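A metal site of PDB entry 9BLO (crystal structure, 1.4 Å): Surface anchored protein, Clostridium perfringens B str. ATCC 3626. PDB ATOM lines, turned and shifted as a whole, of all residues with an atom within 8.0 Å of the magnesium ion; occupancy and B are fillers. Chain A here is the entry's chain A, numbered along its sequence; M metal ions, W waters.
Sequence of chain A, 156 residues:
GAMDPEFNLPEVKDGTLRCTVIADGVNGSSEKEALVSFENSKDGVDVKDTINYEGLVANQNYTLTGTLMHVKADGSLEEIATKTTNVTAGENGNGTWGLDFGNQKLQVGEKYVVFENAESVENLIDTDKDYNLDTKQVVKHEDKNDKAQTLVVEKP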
ATOM      1  N   ILE A 125     -13.114 -25.712 -27.254  1.00  0.00           N
ATOM      2  CA  ILE A 125     -14.164 -26.746 -27.044  1.00  0.00           C
ATOM      3  C   ILE A 125     -13.709 -27.708 -25.936  1.00  0.00           C
ATOM      4  O   ILE A 125     -12.546 -28.143 -25.960  1.00  0.00           O
ATOM      5  CB  ILE A 125     -14.490 -27.471 -28.361  1.00  0.00           C
ATOM      6  CG1 ILE A 125     -14.997 -26.493 -29.421  1.00  0.00           C
ATOM      7  CG2 ILE A 125     -15.459 -28.619 -28.120  1.00  0.00           C
ATOM      8  CD1 ILE A 125     -15.099 -27.090 -30.806  1.00  0.00           C
ATOM      9  N   ASP A 126     -14.617 -28.002 -25.001  1.00  0.00           N
ATOM     10  CA  ASP A 126     -14.431 -29.026 -23.949  1.00  0.00           C
ATOM     11  C   ASP A 126     -15.060 -30.327 -24.443  1.00  0.00           C
ATOM     12  O   ASP A 126     -16.272 -30.329 -24.708  1.00  0.00           O
ATOM     13  CB  ASP A 126     -15.045 -28.554 -22.625  1.00  0.00           C
ATOM     14  CG  ASP A 126     -14.894 -29.559 -21.501  1.00  0.00           C
ATOM     15  OD1 ASP A 126     -13.942 -30.378 -21.543  1.00  0.00           O
ATOM     16  OD2 ASP A 126     -15.751 -29.526 -20.599  1.00  0.00           O
ATOM     17  N   THR A 127     -14.252 -31.383 -24.572  1.00  0.00           N
ATOM     18  CA  THR A 127     -14.651 -32.694 -25.157  1.00  0.00           C
ATOM     19  C   THR A 127     -14.721 -33.787 -24.072  1.00  0.00           C
ATOM     20  O   THR A 127     -15.086 -34.919 -24.445  1.00  0.00           O
ATOM     21  CB  THR A 127     -13.682 -33.139 -26.257  1.00  0.00           C
ATOM     22  OG1 THR A 127     -12.391 -33.339 -25.699  1.00  0.00           O
ATOM     23  CG2 THR A 127     -13.613 -32.145 -27.402  1.00  0.00           C
ATOM     24  N   ASP A 128     -14.397 -33.474 -22.809  1.00  0.00           N
ATOM     25  CA  ASP A 128     -14.303 -34.486 -21.717  1.00  0.00           C
ATOM     26  C   ASP A 128     -15.006 -34.008 -20.442  1.00  0.00           C
ATOM     27  O   ASP A 128     -14.700 -34.562 -19.368  1.00  0.00           O
ATOM     28  CB  ASP A 128     -12.838 -34.877 -21.469  1.00  0.00           C
ATOM     29  CG  ASP A 128     -11.893 -33.710 -21.211  1.00  0.00           C
ATOM     30  OD1 ASP A 128     -12.379 -32.585 -21.002  1.00  0.00           O
ATOM     31  OD2 ASP A 128     -10.665 -33.949 -21.234  1.00  0.00           O
ATOM     32  N   LYS A 129     -15.922 -33.040 -20.558  1.00  0.00           N
ATOM     33  CA  LYS A 129     -16.906 -32.656 -19.501  1.00  0.00           C
ATOM     34  C   LYS A 129     -16.190 -32.204 -18.206  1.00  0.00           C
ATOM     35  O   LYS A 129     -16.727 -32.477 -17.120  1.00  0.00           O
ATOM     36  CB  LYS A 129     -17.868 -33.815 -19.227  1.00  0.00           C
ATOM     37  CG  LYS A 129     -18.639 -34.298 -20.440  1.00  0.00           C
ATOM     38  CD  LYS A 129     -19.201 -35.712 -20.321  1.00  0.00           C
ATOM     39  CE  LYS A 129     -20.570 -35.789 -19.666  1.00  0.00           C
ATOM     40  NZ  LYS A 129     -20.485 -36.244 -18.259  1.00  0.00           N
ATOM     41  N   ASP A 130     -15.050 -31.504 -18.321  1.00  0.00           N
ATOM     42  CA  ASP A 130     -14.263 -31.017 -17.145  1.00  0.00           C
ATOM     43  C   ASP A 130     -14.219 -29.489 -17.116  1.00  0.00           C
ATOM     44  O   ASP A 130     -13.548 -28.942 -16.211  1.00  0.00           O
ATOM     45  CB  ASP A 130     -12.863 -31.648 -17.127  1.00  0.00           C
ATOM     46  CG  ASP A 130     -11.964 -31.250 -18.294  1.00  0.00           C
ATOM     47  OD1 ASP A 130     -12.428 -30.502 -19.181  1.00  0.00           O
ATOM     48  OD2 ASP A 130     -10.805 -31.712 -18.299  1.00  0.00           O
ATOM     49  N   TYR A 131     -14.905 -28.814 -18.042  1.00  0.00           N
ATOM     50  CA  TYR A 131     -14.994 -27.332 -18.184  1.00  0.00           C
ATOM     51  C   TYR A 131     -13.613 -26.734 -18.472  1.00  0.00           C
ATOM     52  O   TYR A 131     -13.461 -25.495 -18.407  1.00  0.00           O
ATOM     53  CB  TYR A 131     -15.659 -26.700 -16.957  1.00  0.00           C
ATOM     54  CG  TYR A 131     -17.150 -26.925 -16.938  1.00  0.00           C
ATOM     55  CD1 TYR A 131     -17.686 -28.100 -16.424  1.00  0.00           C
ATOM     56  CD2 TYR A 131     -18.024 -25.995 -17.478  1.00  0.00           C
ATOM     57  CE1 TYR A 131     -19.056 -28.320 -16.432  1.00  0.00           C
ATOM     58  CE2 TYR A 131     -19.388 -26.208 -17.491  1.00  0.00           C
ATOM     59  CZ  TYR A 131     -19.907 -27.374 -16.965  1.00  0.00           C
ATOM     60  OH  TYR A 131     -21.259 -27.599 -16.961  1.00  0.00           O
ATOM     61  N   ASN A 132     -12.635 -27.581 -18.815  1.00  0.00           N
ATOM     62  CA  ASN A 132     -11.329 -27.171 -19.371  1.00  0.00           C
ATOM     63  C   ASN A 132     -11.404 -27.345 -20.883  1.00  0.00           C
ATOM     64  O   ASN A 132     -11.619 -28.499 -21.350  1.00  0.00           O
ATOM     65  CB  ASN A 132     -10.162 -27.958 -18.778  1.00  0.00           C
ATOM     66  CG  ASN A 132      -8.858 -27.662 -19.478  1.00  0.00           C
ATOM     67  OD1 ASN A 132      -8.291 -26.576 -19.320  1.00  0.00           O
ATOM     68  ND2 ASN A 132      -8.372 -28.602 -20.272  1.00  0.00           N
ATOM     69  N   LEU A 133     -11.273 -26.237 -21.630  1.00  0.00           N
ATOM     70  CA  LEU A 133     -11.269 -26.247 -23.110  1.00  0.00           C
ATOM     71  C   LEU A 133      -9.982 -26.959 -23.559  1.00  0.00           C
ATOM     72  O   LEU A 133      -8.902 -26.588 -23.075  1.00  0.00           O
ATOM     73  CB  LEU A 133     -11.338 -24.809 -23.645  1.00  0.00           C
ATOM     74  CG  LEU A 133     -12.516 -23.972 -23.143  1.00  0.00           C
ATOM     75  CD1 LEU A 133     -12.491 -22.588 -23.776  1.00  0.00           C
ATOM     76  CD2 LEU A 133     -13.836 -24.667 -23.445  1.00  0.00           C
ATOM     77  N   ASP A 134     -10.118 -27.963 -24.427  1.00  0.00           N
ATOM     78  CA  ASP A 134      -9.039 -28.934 -24.713  1.00  0.00           C
ATOM     79  C   ASP A 134      -8.884 -29.194 -26.219  1.00  0.00           C
ATOM     80  O   ASP A 134      -7.892 -29.864 -26.584  1.00  0.00           O
ATOM     81  CB  ASP A 134      -9.310 -30.235 -23.963  1.00  0.00           C
ATOM     82  CG  ASP A 134     -10.712 -30.778 -24.201  1.00  0.00           C
ATOM     83  OD1 ASP A 134     -11.015 -31.137 -25.361  1.00  0.00           O
ATOM     84  OD2 ASP A 134     -11.501 -30.813 -23.240  1.00  0.00           O
ATOM     85  N   THR A 135      -9.790 -28.694 -27.061  1.00  0.00           N
ATOM     86  CA  THR A 135      -9.856 -29.018 -28.509  1.00  0.00           C
ATOM     87  C   THR A 135     -10.088 -27.730 -29.315  1.00  0.00           C
ATOM     88  O   THR A 135     -10.902 -26.900 -28.878  1.00  0.00           O
ATOM     89  CB  THR A 135     -10.954 -30.054 -28.788  1.00  0.00           C
ATOM     90  OG1 THR A 135     -10.642 -31.221 -28.031  1.00  0.00           O
ATOM     91  CG2 THR A 135     -11.063 -30.424 -30.248  1.00  0.00           C
HETATM   92 MG    MG M   1     -11.897 -30.571 -21.197  1.00  0.00          MG
HETATM   93  O   HOH W   1      -9.891 -30.854 -20.734  1.00  0.00           O
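N of Tyr 131 is in hydrogen-bond range of OD2 of Asp 126 (2.8 Å).
The backbone carbonyl oxygen of Ile 125 lies within hydrogen-bond range of the backbone NH of Asp 134 (2.9 Å).
OD1 of Asp 134 lies within hydrogen-bond range of OG1 of Thr 135, at 2.7 Å.
OG1 of Thr 127 lies within hydrogen-bond range of OD1 of Asp 134, 2.6 Å away.
OD1 of Asp 126 sits close to N of Lys 129.
The nearest printed residue that does not touch the magnesium ion is Thr 127 (4.2 Å).
The magnesium ion is bound by water W1 (2.1 Å), the side-chain carboxylate of Asp 128 (2.1 Å), the side-chain carboxylate of Asp 126 (2.1 Å), the side-chain carboxylate of Asp 130 (2.1 Å), the side-chain carboxylate of Asp 134 (2.1 Å) and the backbone carbonyl oxygen of Asn 132 (2.1 Å).
Water W1 lies within hydrogen-bond range of OD2 of Asp 130 (2.7 Å), ND2 of Asn 132 (2.8 Å) and OD2 of Asp 128 (3.2 Å).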
